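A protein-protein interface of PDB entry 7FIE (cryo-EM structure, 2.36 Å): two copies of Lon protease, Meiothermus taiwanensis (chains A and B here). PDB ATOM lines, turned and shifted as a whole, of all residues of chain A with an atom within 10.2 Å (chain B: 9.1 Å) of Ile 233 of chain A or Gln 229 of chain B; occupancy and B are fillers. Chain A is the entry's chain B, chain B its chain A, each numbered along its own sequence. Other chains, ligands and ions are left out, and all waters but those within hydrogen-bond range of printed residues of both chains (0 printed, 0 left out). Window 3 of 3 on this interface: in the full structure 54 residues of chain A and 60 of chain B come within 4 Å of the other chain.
Among the printed residues, pairs that only touch across the chains: Leu 226 of chain A with Glu 236 of chain B (3.3 Å), Ile 233 of chain A with Leu 226 of chain B (3.5 Å), Leu 226 of chain A with Ile 233 of chain B (3.7 Å), Ile 233 of chain A with Met 230 of chain B (3.7 Å), Leu 237 of chain A with Leu 226 of chain B (3.7 Å), Leu 237 of chain A with Glu 223 of chain B (3.8 Å), Met 230 of chain A with Met 230 of chain B (3.8 Å) and Ile 233 of chain A with Gln 229 of chain B (3.9 Å).
The guanidinium group (NH1) of Arg 227 of chain B lies within salt-bridge range of the side-chain carboxylate (OE2) of Glu 223 of chain B, at 3.7 Å. O of Tyr 225 of chain B sits close to OE1 of Gln 229 of chain B (2.8 Å).
Of the 19 printed residues of chain A, 4 touch a printed residue of chain B. Printed residues of chain B that touch a printed residue of chain A: Glu 223, Leu 226, Gln 229, Met 230, Ile 233 and Glu 236. Along chain B the printed residues that touch a printed residue of chain A span positions 223 to 236. Among the printed residues, no Asp or Glu carboxylate lies within 4 Å of a Lys or Arg side-chain nitrogen of the other chain.
No residue of chain B comes within 4 Å of Ala 232 of chain A. Ile 233 of chain A touches just these residues of chain B: Leu 226 (3.5 Å), Gln 229 (3.9 Å) and Met 230 (3.7 Å). Of the printed residues of chain B, Leu 237 of chain A touches Glu 223 and Leu 226. Of the printed residues of chain A, Glu 223 of chain B touches Leu 237. No residue of chain A comes within 4 Å of Tyr 225 of chain B. Of chain A, only Ile 233 and Leu 237 come within 4 Å of Leu 226 of chain B. Gln 229 of chain B touches just one residue of chain A: Ile 233. No residue of chain A comes within 4 Å of Ala 232 of chain B. Ile 233 of chain B touches one residue of chain A. Of the printed residues of chain A, Glu 236 of chain B touches Leu 226 (3.3 Å). The nearest residue of chain A that does not touch Gln 229 of chain B is Gln 229 of chain A (7.2 Å).
Leu 226 of chain A touches Ile 233 of chain B, and with the chains exchanged Ile 233 of chain A touches Leu 226 of chain B. Leu 226 of chain A touches Glu 236 of chain B, but with the chains exchanged Glu 236 of chain A does not touch Leu 226 of chain B (4.2 Å). Met 230 of chain A touches its own counterpart, Met 230 of chain B. Ile 233 of chain A touches Met 230 of chain B, but with the chains exchanged Met 230 of chain A does not touch Ile 233 of chain B (4.7 Å).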
ATOM      1  N   TYR A 225     -17.154   2.141   6.182  1.00  0.00           N
ATOM      2  CA  TYR A 225     -15.983   1.284   6.345  1.00  0.00           C
ATOM      3  C   TYR A 225     -16.249   0.187   7.372  1.00  0.00           C
ATOM      4  O   TYR A 225     -15.754  -0.939   7.234  1.00  0.00           O
ATOM      5  CB  TYR A 225     -14.781   2.149   6.717  1.00  0.00           C
ATOM      6  CG  TYR A 225     -13.450   1.440   6.704  1.00  0.00           C
ATOM      7  CD1 TYR A 225     -12.991   0.834   5.542  1.00  0.00           C
ATOM      8  CD2 TYR A 225     -12.599   1.472   7.806  1.00  0.00           C
ATOM      9  CE1 TYR A 225     -11.764   0.202   5.495  1.00  0.00           C
ATOM     10  CE2 TYR A 225     -11.352   0.858   7.762  1.00  0.00           C
ATOM     11  CZ  TYR A 225     -10.949   0.217   6.604  1.00  0.00           C
ATOM     12  OH  TYR A 225      -9.729  -0.412   6.546  1.00  0.00           O
ATOM     13  N   LEU A 226     -17.070   0.491   8.376  1.00  0.00           N
ATOM     14  CA  LEU A 226     -17.612  -0.546   9.249  1.00  0.00           C
ATOM     15  C   LEU A 226     -18.480  -1.532   8.467  1.00  0.00           C
ATOM     16  O   LEU A 226     -18.473  -2.745   8.741  1.00  0.00           O
ATOM     17  CB  LEU A 226     -18.412   0.110  10.368  1.00  0.00           C
ATOM     18  CG  LEU A 226     -18.992  -0.804  11.442  1.00  0.00           C
ATOM     19  CD1 LEU A 226     -17.853  -1.434  12.200  1.00  0.00           C
ATOM     20  CD2 LEU A 226     -19.942  -0.069  12.390  1.00  0.00           C
ATOM     21  N   ARG A 227     -19.237  -1.025   7.493  1.00  0.00           N
ATOM     22  CA  ARG A 227     -19.990  -1.909   6.605  1.00  0.00           C
ATOM     23  C   ARG A 227     -19.065  -2.754   5.737  1.00  0.00           C
ATOM     24  O   ARG A 227     -19.391  -3.897   5.405  1.00  0.00           O
ATOM     25  CB  ARG A 227     -20.953  -1.110   5.728  1.00  0.00           C
ATOM     26  CG  ARG A 227     -21.990  -0.361   6.518  1.00  0.00           C
ATOM     27  CD  ARG A 227     -22.920  -1.304   7.250  1.00  0.00           C
ATOM     28  NE  ARG A 227     -23.838  -0.564   8.113  1.00  0.00           N
ATOM     29  CZ  ARG A 227     -25.020  -0.099   7.723  1.00  0.00           C
ATOM     30  NH1 ARG A 227     -25.429  -0.293   6.481  1.00  0.00           N
ATOM     31  NH2 ARG A 227     -25.795   0.558   8.574  1.00  0.00           N
ATOM     32  N   GLU A 228     -17.913  -2.196   5.350  1.00  0.00           N
ATOM     33  CA  GLU A 228     -16.892  -2.973   4.646  1.00  0.00           C
ATOM     34  C   GLU A 228     -16.377  -4.131   5.499  1.00  0.00           C
ATOM     35  O   GLU A 228     -16.195  -5.248   4.991  1.00  0.00           O
ATOM     36  CB  GLU A 228     -15.737  -2.058   4.223  1.00  0.00           C
ATOM     37  CG  GLU A 228     -14.526  -2.743   3.566  1.00  0.00           C
ATOM     38  CD  GLU A 228     -14.783  -3.261   2.163  1.00  0.00           C
ATOM     39  OE1 GLU A 228     -15.669  -2.723   1.467  1.00  0.00           O
ATOM     40  OE2 GLU A 228     -14.082  -4.208   1.745  1.00  0.00           O
ATOM     41  N   GLN A 229     -16.152  -3.898   6.798  1.00  0.00           N
ATOM     42  CA  GLN A 229     -15.689  -5.006   7.637  1.00  0.00           C
ATOM     43  C   GLN A 229     -16.774  -6.059   7.838  1.00  0.00           C
ATOM     44  O   GLN A 229     -16.490  -7.268   7.799  1.00  0.00           O
ATOM     45  CB  GLN A 229     -15.161  -4.536   8.996  1.00  0.00           C
ATOM     46  CG  GLN A 229     -13.750  -3.995   8.935  1.00  0.00           C
ATOM     47  CD  GLN A 229     -13.691  -2.498   8.940  1.00  0.00           C
ATOM     48  OE1 GLN A 229     -14.493  -1.835   9.589  1.00  0.00           O
ATOM     49  NE2 GLN A 229     -12.784  -1.949   8.157  1.00  0.00           N
ATOM     50  N   MET A 230     -18.024  -5.632   8.036  1.00  0.00           N
ATOM     51  CA  MET A 230     -19.074  -6.625   8.247  1.00  0.00           C
ATOM     52  C   MET A 230     -19.387  -7.360   6.945  1.00  0.00           C
ATOM     53  O   MET A 230     -19.766  -8.536   6.959  1.00  0.00           O
ATOM     54  CB  MET A 230     -20.323  -5.981   8.861  1.00  0.00           C
ATOM     55  CG  MET A 230     -21.176  -5.132   7.946  1.00  0.00           C
ATOM     56  SD  MET A 230     -22.514  -6.045   7.156  1.00  0.00           S
ATOM     57  CE  MET A 230     -22.705  -5.083   5.665  1.00  0.00           C
ATOM     58  N   LYS A 231     -19.135  -6.709   5.804  1.00  0.00           N
ATOM     59  CA  LYS A 231     -19.249  -7.377   4.511  1.00  0.00           C
ATOM     60  C   LYS A 231     -18.145  -8.410   4.332  1.00  0.00           C
ATOM     61  O   LYS A 231     -18.375  -9.462   3.729  1.00  0.00           O
ATOM     62  CB  LYS A 231     -19.197  -6.334   3.388  1.00  0.00           C
ATOM     63  CG  LYS A 231     -19.310  -6.861   1.947  1.00  0.00           C
ATOM     64  CD  LYS A 231     -17.950  -6.960   1.259  1.00  0.00           C
ATOM     65  CE  LYS A 231     -17.355  -5.582   1.081  1.00  0.00           C
ATOM     66  NZ  LYS A 231     -16.002  -5.659   0.477  1.00  0.00           N
ATOM     67  N   ALA A 232     -16.938  -8.103   4.827  1.00  0.00           N
ATOM     68  CA  ALA A 232     -15.828  -9.050   4.772  1.00  0.00           C
ATOM     69  C   ALA A 232     -16.140 -10.300   5.584  1.00  0.00           C
ATOM     70  O   ALA A 232     -16.002 -11.436   5.091  1.00  0.00           O
ATOM     71  CB  ALA A 232     -14.540  -8.398   5.274  1.00  0.00           C
ATOM     72  N   ILE A 233     -16.612 -10.094   6.820  1.00  0.00           N
ATOM     73  CA  ILE A 233     -17.007 -11.196   7.696  1.00  0.00           C
ATOM     74  C   ILE A 233     -18.164 -11.979   7.088  1.00  0.00           C
ATOM     75  O   ILE A 233     -18.190 -13.214   7.157  1.00  0.00           O
ATOM     76  CB  ILE A 233     -17.355 -10.652   9.097  1.00  0.00           C
ATOM     77  CG1 ILE A 233     -16.155  -9.934   9.709  1.00  0.00           C
ATOM     78  CG2 ILE A 233     -17.783 -11.773  10.035  1.00  0.00           C
ATOM     79  CD1 ILE A 233     -16.491  -9.103  10.942  1.00  0.00           C
ATOM     80  N   GLN A 234     -19.104 -11.289   6.439  1.00  0.00           N
ATOM     81  CA  GLN A 234     -20.249 -11.951   5.832  1.00  0.00           C
ATOM     82  C   GLN A 234     -19.870 -12.784   4.615  1.00  0.00           C
ATOM     83  O   GLN A 234     -20.351 -13.913   4.483  1.00  0.00           O
ATOM     84  CB  GLN A 234     -21.304 -10.907   5.451  1.00  0.00           C
ATOM     85  CG  GLN A 234     -22.602 -11.465   4.842  1.00  0.00           C
ATOM     86  CD  GLN A 234     -23.384 -12.366   5.784  1.00  0.00           C
ATOM     87  OE1 GLN A 234     -23.396 -13.583   5.625  1.00  0.00           O
ATOM     88  NE2 GLN A 234     -24.043 -11.770   6.768  1.00  0.00           N
ATOM     89  N   LYS A 235     -19.022 -12.277   3.719  1.00  0.00           N
ATOM     90  CA  LYS A 235     -18.810 -13.053   2.505  1.00  0.00           C
ATOM     91  C   LYS A 235     -17.732 -14.106   2.687  1.00  0.00           C
ATOM     92  O   LYS A 235     -17.624 -15.014   1.852  1.00  0.00           O
ATOM     93  CB  LYS A 235     -18.469 -12.166   1.295  1.00  0.00           C
ATOM     94  CG  LYS A 235     -16.990 -11.995   0.922  1.00  0.00           C
ATOM     95  CD  LYS A 235     -16.232 -11.003   1.758  1.00  0.00           C
ATOM     96  CE  LYS A 235     -14.898 -10.641   1.102  1.00  0.00           C
ATOM     97  NZ  LYS A 235     -14.072  -9.744   1.953  1.00  0.00           N
ATOM     98  N   GLU A 236     -16.941 -14.037   3.762  1.00  0.00           N
ATOM     99  CA  GLU A 236     -16.008 -15.129   3.995  1.00  0.00           C
ATOM    100  C   GLU A 236     -16.669 -16.342   4.655  1.00  0.00           C
ATOM    101  O   GLU A 236     -16.090 -17.433   4.643  1.00  0.00           O
ATOM    102  CB  GLU A 236     -14.798 -14.615   4.796  1.00  0.00           C
ATOM    103  CG  GLU A 236     -13.580 -15.548   4.812  1.00  0.00           C
ATOM    104  CD  GLU A 236     -13.050 -15.878   3.411  1.00  0.00           C
ATOM    105  OE1 GLU A 236     -13.124 -15.026   2.497  1.00  0.00           O
ATOM    106  OE2 GLU A 236     -12.590 -17.023   3.215  1.00  0.00           O
ATOM    107  N   LEU A 237     -17.927 -16.141   5.054  1.00  0.00           N
ATOM    108  CA  LEU A 237     -18.745 -17.234   5.630  1.00  0.00           C
ATOM    109  C   LEU A 237     -20.100 -17.135   4.926  1.00  0.00           C
ATOM    110  O   LEU A 237     -21.096 -17.603   5.507  1.00  0.00           O
ATOM    111  CB  LEU A 237     -18.923 -16.944   7.122  1.00  0.00           C
ATOM    112  CG  LEU A 237     -17.803 -17.431   8.038  1.00  0.00           C
ATOM    113  CD1 LEU A 237     -18.248 -17.367   9.491  1.00  0.00           C
ATOM    114  CD2 LEU A 237     -17.385 -18.846   7.673  1.00  0.00           C
ATOM    115  N   GLY A 238     -20.133 -16.551   3.723  1.00  0.00           N
ATOM    116  CA  GLY A 238     -21.417 -16.296   3.028  1.00  0.00           C
ATOM    117  C   GLY A 238     -22.196 -17.533   2.634  1.00  0.00           C
ATOM    118  O   GLY A 238     -21.562 -18.518   2.209  1.00  0.00           O
ATOM    119  N   GLY A 239     -23.527 -17.483   2.760  1.00  0.00           N
ATOM    120  CA  GLY A 239     -24.380 -18.607   2.325  1.00  0.00           C
ATOM    121  C   GLY A 239     -25.126 -18.274   1.045  1.00  0.00           C
ATOM    122  O   GLY A 239     -26.069 -19.021   0.734  1.00  0.00           O
ATOM    123  N   ASP A 241     -26.900 -15.860   0.920  1.00  0.00           N
ATOM    124  CA  ASP A 241     -28.158 -15.386   1.543  1.00  0.00           C
ATOM    125  C   ASP A 241     -27.713 -14.709   2.829  1.00  0.00           C
ATOM    126  O   ASP A 241     -26.492 -14.647   3.047  1.00  0.00           O
ATOM    127  CB  ASP A 241     -29.162 -16.525   1.737  1.00  0.00           C
ATOM    128  CG  ASP A 241     -28.772 -17.581   2.759  1.00  0.00           C
ATOM    129  OD1 ASP A 241     -27.586 -17.640   3.135  1.00  0.00           O
ATOM    130  OD2 ASP A 241     -29.668 -18.348   3.165  1.00  0.00           O
ATOM    131  N   GLY A 242     -28.631 -14.191   3.633  1.00  0.00           N
ATOM    132  CA  GLY A 242     -28.151 -13.611   4.899  1.00  0.00           C
ATOM    133  C   GLY A 242     -27.730 -12.188   4.642  1.00  0.00           C
ATOM    134  O   GLY A 242     -27.339 -11.504   5.604  1.00  0.00           O
ATOM    135  N   LEU A 243     -27.845 -11.760   3.390  1.00  0.00           N
ATOM    136  CA  LEU A 243     -27.525 -10.370   3.006  1.00  0.00           C
ATOM    137  C   LEU A 243     -27.861 -10.345   1.529  1.00  0.00           C
ATOM    138  O   LEU A 243     -27.895  -9.262   0.924  1.00  0.00           O
ATOM    139  CB  LEU A 243     -26.036 -10.100   3.225  1.00  0.00           C
ATOM    140  CG  LEU A 243     -25.654  -8.620   3.252  1.00  0.00           C
ATOM    141  CD1 LEU A 243     -26.480  -7.872   4.286  1.00  0.00           C
ATOM    142  CD2 LEU A 243     -24.169  -8.439   3.518  1.00  0.00           C
ATOM    143  N   GLN A 277     -28.959 -17.208  12.668  1.00  0.00           N
ATOM    144  CA  GLN A 277     -27.819 -17.490  11.791  1.00  0.00           C
ATOM    145  C   GLN A 277     -27.984 -18.705  10.880  1.00  0.00           C
ATOM    146  O   GLN A 277     -27.016 -19.089  10.214  1.00  0.00           O
ATOM    147  CB  GLN A 277     -26.550 -17.682  12.623  1.00  0.00           C
ATOM    148  CG  GLN A 277     -26.032 -16.421  13.277  1.00  0.00           C
ATOM    149  CD  GLN A 277     -25.678 -15.369  12.260  1.00  0.00           C
ATOM    150  OE1 GLN A 277     -26.315 -14.321  12.185  1.00  0.00           O
ATOM    151  NE2 GLN A 277     -24.670 -15.655  11.446  1.00  0.00           N
ATOM    152  N   GLN B 221     -12.790 -23.440  13.866  1.00  0.00           N
ATOM    153  CA  GLN B 221     -12.173 -22.419  14.710  1.00  0.00           C
ATOM    154  C   GLN B 221     -12.044 -21.096  13.955  1.00  0.00           C
ATOM    155  O   GLN B 221     -12.106 -20.019  14.568  1.00  0.00           O
ATOM    156  CB  GLN B 221     -10.821 -22.894  15.252  1.00  0.00           C
ATOM    157  CG  GLN B 221      -9.653 -22.916  14.273  1.00  0.00           C
ATOM    158  CD  GLN B 221      -8.864 -21.620  14.286  1.00  0.00           C
ATOM    159  OE1 GLN B 221      -8.768 -20.953  15.316  1.00  0.00           O
ATOM    160  NE2 GLN B 221      -8.322 -21.246  13.137  1.00  0.00           N
ATOM    161  N   ARG B 222     -11.926 -21.169  12.624  1.00  0.00           N
ATOM    162  CA  ARG B 222     -11.987 -20.015  11.744  1.00  0.00           C
ATOM    163  C   ARG B 222     -13.315 -19.293  11.872  1.00  0.00           C
ATOM    164  O   ARG B 222     -13.337 -18.071  12.010  1.00  0.00           O
ATOM    165  CB  ARG B 222     -11.790 -20.476  10.300  1.00  0.00           C
ATOM    166  CG  ARG B 222     -11.852 -19.395   9.237  1.00  0.00           C
ATOM    167  CD  ARG B 222     -10.499 -18.782   8.931  1.00  0.00           C
ATOM    168  NE  ARG B 222     -10.108 -17.665   9.758  1.00  0.00           N
ATOM    169  CZ  ARG B 222      -8.903 -17.112   9.710  1.00  0.00           C
ATOM    170  NH1 ARG B 222      -7.986 -17.589   8.881  1.00  0.00           N
ATOM    171  NH2 ARG B 222      -8.612 -16.082  10.498  1.00  0.00           N
ATOM    172  N   GLU B 223     -14.429 -20.032  11.850  1.00  0.00           N
ATOM    173  CA  GLU B 223     -15.731 -19.372  11.900  1.00  0.00           C
ATOM    174  C   GLU B 223     -16.015 -18.829  13.297  1.00  0.00           C
ATOM    175  O   GLU B 223     -16.695 -17.803  13.438  1.00  0.00           O
ATOM    176  CB  GLU B 223     -16.845 -20.317  11.435  1.00  0.00           C
ATOM    177  CG  GLU B 223     -17.218 -21.429  12.397  1.00  0.00           C
ATOM    178  CD  GLU B 223     -18.294 -22.348  11.870  1.00  0.00           C
ATOM    179  OE1 GLU B 223     -18.762 -22.146  10.728  1.00  0.00           O
ATOM    180  OE2 GLU B 223     -18.669 -23.280  12.613  1.00  0.00           O
ATOM    181  N   TYR B 224     -15.472 -19.484  14.339  1.00  0.00           N
ATOM    182  CA  TYR B 224     -15.535 -18.908  15.679  1.00  0.00           C
ATOM    183  C   TYR B 224     -14.812 -17.574  15.725  1.00  0.00           C
ATOM    184  O   TYR B 224     -15.359 -16.586  16.226  1.00  0.00           O
ATOM    185  CB  TYR B 224     -14.933 -19.856  16.712  1.00  0.00           C
ATOM    186  CG  TYR B 224     -14.859 -19.238  18.093  1.00  0.00           C
ATOM    187  CD1 TYR B 224     -15.996 -19.105  18.877  1.00  0.00           C
ATOM    188  CD2 TYR B 224     -13.650 -18.775  18.607  1.00  0.00           C
ATOM    189  CE1 TYR B 224     -15.931 -18.535  20.131  1.00  0.00           C
ATOM    190  CE2 TYR B 224     -13.580 -18.198  19.851  1.00  0.00           C
ATOM    191  CZ  TYR B 224     -14.720 -18.084  20.608  1.00  0.00           C
ATOM    192  OH  TYR B 224     -14.641 -17.514  21.855  1.00  0.00           O
ATOM    193  N   TYR B 225     -13.587 -17.544  15.190  1.00  0.00           N
ATOM    194  CA  TYR B 225     -12.791 -16.324  15.095  1.00  0.00           C
ATOM    195  C   TYR B 225     -13.522 -15.241  14.311  1.00  0.00           C
ATOM    196  O   TYR B 225     -13.550 -14.073  14.718  1.00  0.00           O
ATOM    197  CB  TYR B 225     -11.470 -16.685  14.423  1.00  0.00           C
ATOM    198  CG  TYR B 225     -10.410 -15.621  14.353  1.00  0.00           C
ATOM    199  CD1 TYR B 225      -9.611 -15.339  15.451  1.00  0.00           C
ATOM    200  CD2 TYR B 225     -10.175 -14.931  13.172  1.00  0.00           C
ATOM    201  CE1 TYR B 225      -8.619 -14.381  15.384  1.00  0.00           C
ATOM    202  CE2 TYR B 225      -9.183 -13.977  13.087  1.00  0.00           C
ATOM    203  CZ  TYR B 225      -8.402 -13.707  14.196  1.00  0.00           C
ATOM    204  OH  TYR B 225      -7.425 -12.741  14.125  1.00  0.00           O
ATOM    205  N   LEU B 226     -14.188 -15.632  13.224  1.00  0.00           N
ATOM    206  CA  LEU B 226     -14.824 -14.663  12.341  1.00  0.00           C
ATOM    207  C   LEU B 226     -16.073 -14.047  12.956  1.00  0.00           C
ATOM    208  O   LEU B 226     -16.214 -12.818  12.944  1.00  0.00           O
ATOM    209  CB  LEU B 226     -15.149 -15.306  10.991  1.00  0.00           C
ATOM    210  CG  LEU B 226     -13.944 -15.549  10.081  1.00  0.00           C
ATOM    211  CD1 LEU B 226     -14.336 -16.336   8.843  1.00  0.00           C
ATOM    212  CD2 LEU B 226     -13.299 -14.230   9.704  1.00  0.00           C
ATOM    213  N   ARG B 227     -16.985 -14.842  13.529  1.00  0.00           N
ATOM    214  CA  ARG B 227     -18.077 -14.109  14.163  1.00  0.00           C
ATOM    215  C   ARG B 227     -17.708 -13.642  15.565  1.00  0.00           C
ATOM    216  O   ARG B 227     -18.461 -12.874  16.169  1.00  0.00           O
ATOM    217  CB  ARG B 227     -19.424 -14.854  14.157  1.00  0.00           C
ATOM    218  CG  ARG B 227     -19.708 -15.956  15.154  1.00  0.00           C
ATOM    219  CD  ARG B 227     -19.708 -17.313  14.505  1.00  0.00           C
ATOM    220  NE  ARG B 227     -20.408 -18.280  15.342  1.00  0.00           N
ATOM    221  CZ  ARG B 227     -20.486 -19.577  15.082  1.00  0.00           C
ATOM    222  NH1 ARG B 227     -19.913 -20.064  13.994  1.00  0.00           N
ATOM    223  NH2 ARG B 227     -21.149 -20.381  15.901  1.00  0.00           N
ATOM    224  N   GLU B 228     -16.519 -13.988  16.053  1.00  0.00           N
ATOM    225  CA  GLU B 228     -15.975 -13.276  17.198  1.00  0.00           C
ATOM    226  C   GLU B 228     -15.626 -11.844  16.808  1.00  0.00           C
ATOM    227  O   GLU B 228     -15.927 -10.894  17.547  1.00  0.00           O
ATOM    228  CB  GLU B 228     -14.749 -14.023  17.716  1.00  0.00           C
ATOM    229  CG  GLU B 228     -14.324 -13.705  19.116  1.00  0.00           C
ATOM    230  CD  GLU B 228     -15.215 -14.340  20.148  1.00  0.00           C
ATOM    231  OE1 GLU B 228     -15.922 -15.314  19.816  1.00  0.00           O
ATOM    232  OE2 GLU B 228     -15.175 -13.911  21.314  1.00  0.00           O
ATOM    233  N   GLN B 229     -15.022 -11.666  15.626  1.00  0.00           N
ATOM    234  CA  GLN B 229     -14.812 -10.307  15.133  1.00  0.00           C
ATOM    235  C   GLN B 229     -16.129  -9.631  14.780  1.00  0.00           C
ATOM    236  O   GLN B 229     -16.255  -8.415  14.931  1.00  0.00           O
ATOM    237  CB  GLN B 229     -13.861 -10.258  13.935  1.00  0.00           C
ATOM    238  CG  GLN B 229     -12.387 -10.314  14.314  1.00  0.00           C
ATOM    239  CD  GLN B 229     -11.737 -11.647  14.086  1.00  0.00           C
ATOM    240  OE1 GLN B 229     -12.042 -12.352  13.127  1.00  0.00           O
ATOM    241  NE2 GLN B 229     -10.875 -12.030  15.006  1.00  0.00           N
ATOM    242  N   MET B 230     -17.132 -10.401  14.341  1.00  0.00           N
ATOM    243  CA  MET B 230     -18.448  -9.808  14.087  1.00  0.00           C
ATOM    244  C   MET B 230     -19.093  -9.286  15.368  1.00  0.00           C
ATOM    245  O   MET B 230     -19.674  -8.199  15.375  1.00  0.00           O
ATOM    246  CB  MET B 230     -19.379 -10.804  13.393  1.00  0.00           C
ATOM    247  CG  MET B 230     -20.796 -10.270  13.153  1.00  0.00           C
ATOM    248  SD  MET B 230     -20.905  -8.849  12.045  1.00  0.00           S
ATOM    249  CE  MET B 230     -20.805  -9.646  10.446  1.00  0.00           C
ATOM    250  N   LYS B 231     -18.985 -10.022  16.468  1.00  0.00           N
ATOM    251  CA  LYS B 231     -19.568  -9.514  17.702  1.00  0.00           C
ATOM    252  C   LYS B 231     -18.731  -8.401  18.324  1.00  0.00           C
ATOM    253  O   LYS B 231     -19.284  -7.531  19.010  1.00  0.00           O
ATOM    254  CB  LYS B 231     -19.787 -10.673  18.669  1.00  0.00           C
ATOM    255  CG  LYS B 231     -20.808 -11.656  18.111  1.00  0.00           C
ATOM    256  CD  LYS B 231     -21.005 -12.892  18.963  1.00  0.00           C
ATOM    257  CE  LYS B 231     -21.904 -13.874  18.216  1.00  0.00           C
ATOM    258  NZ  LYS B 231     -22.173 -15.163  18.910  1.00  0.00           N
ATOM    259  N   ALA B 232     -17.422  -8.379  18.057  1.00  0.00           N
ATOM    260  CA  ALA B 232     -16.629  -7.203  18.405  1.00  0.00           C
ATOM    261  C   ALA B 232     -17.037  -5.988  17.580  1.00  0.00           C
ATOM    262  O   ALA B 232     -16.954  -4.854  18.064  1.00  0.00           O
ATOM    263  CB  ALA B 232     -15.143  -7.495  18.215  1.00  0.00           C
ATOM    264  N   ILE B 233     -17.446  -6.204  16.330  1.00  0.00           N
ATOM    265  CA  ILE B 233     -18.040  -5.137  15.530  1.00  0.00           C
ATOM    266  C   ILE B 233     -19.383  -4.723  16.120  1.00  0.00           C
ATOM    267  O   ILE B 233     -19.748  -3.540  16.131  1.00  0.00           O
ATOM    268  CB  ILE B 233     -18.157  -5.594  14.061  1.00  0.00           C
ATOM    269  CG1 ILE B 233     -16.775  -5.684  13.408  1.00  0.00           C
ATOM    270  CG2 ILE B 233     -19.110  -4.746  13.239  1.00  0.00           C
ATOM    271  CD1 ILE B 233     -15.981  -4.412  13.435  1.00  0.00           C
ATOM    272  N   GLN B 234     -20.107  -5.691  16.682  1.00  0.00           N
ATOM    273  CA  GLN B 234     -21.382  -5.397  17.323  1.00  0.00           C
ATOM    274  C   GLN B 234     -21.183  -4.632  18.630  1.00  0.00           C
ATOM    275  O   GLN B 234     -22.112  -3.979  19.113  1.00  0.00           O
ATOM    276  CB  GLN B 234     -22.150  -6.696  17.561  1.00  0.00           C
ATOM    277  CG  GLN B 234     -23.620  -6.492  17.814  1.00  0.00           C
ATOM    278  CD  GLN B 234     -24.283  -5.827  16.638  1.00  0.00           C
ATOM    279  OE1 GLN B 234     -24.634  -4.649  16.680  1.00  0.00           O
ATOM    280  NE2 GLN B 234     -24.428  -6.576  15.558  1.00  0.00           N
ATOM    281  N   LYS B 235     -19.961  -4.641  19.181  1.00  0.00           N
ATOM    282  CA  LYS B 235     -19.621  -3.704  20.254  1.00  0.00           C
ATOM    283  C   LYS B 235     -19.446  -2.267  19.750  1.00  0.00           C
ATOM    284  O   LYS B 235     -19.151  -1.369  20.546  1.00  0.00           O
ATOM    285  CB  LYS B 235     -18.355  -4.160  20.974  1.00  0.00           C
ATOM    286  CG  LYS B 235     -18.557  -5.392  21.825  1.00  0.00           C
ATOM    287  CD  LYS B 235     -17.249  -5.839  22.431  1.00  0.00           C
ATOM    288  CE  LYS B 235     -16.768  -4.869  23.488  1.00  0.00           C
ATOM    289  NZ  LYS B 235     -15.542  -5.393  24.142  1.00  0.00           N
ATOM    290  N   GLU B 236     -19.445  -2.106  18.433  1.00  0.00           N
ATOM    291  CA  GLU B 236     -19.235  -0.755  17.866  1.00  0.00           C
ATOM    292  C   GLU B 236     -20.231  -0.572  16.728  1.00  0.00           C
ATOM    293  O   GLU B 236     -19.848  -0.008  15.688  1.00  0.00           O
ATOM    294  CB  GLU B 236     -17.772  -0.516  17.489  1.00  0.00           C
ATOM    295  CG  GLU B 236     -17.161  -1.578  16.596  1.00  0.00           C
ATOM    296  CD  GLU B 236     -15.819  -1.162  16.022  1.00  0.00           C
ATOM    297  OE1 GLU B 236     -15.388  -1.769  15.028  1.00  0.00           O
ATOM    298  OE2 GLU B 236     -15.212  -0.220  16.569  1.00  0.00           O
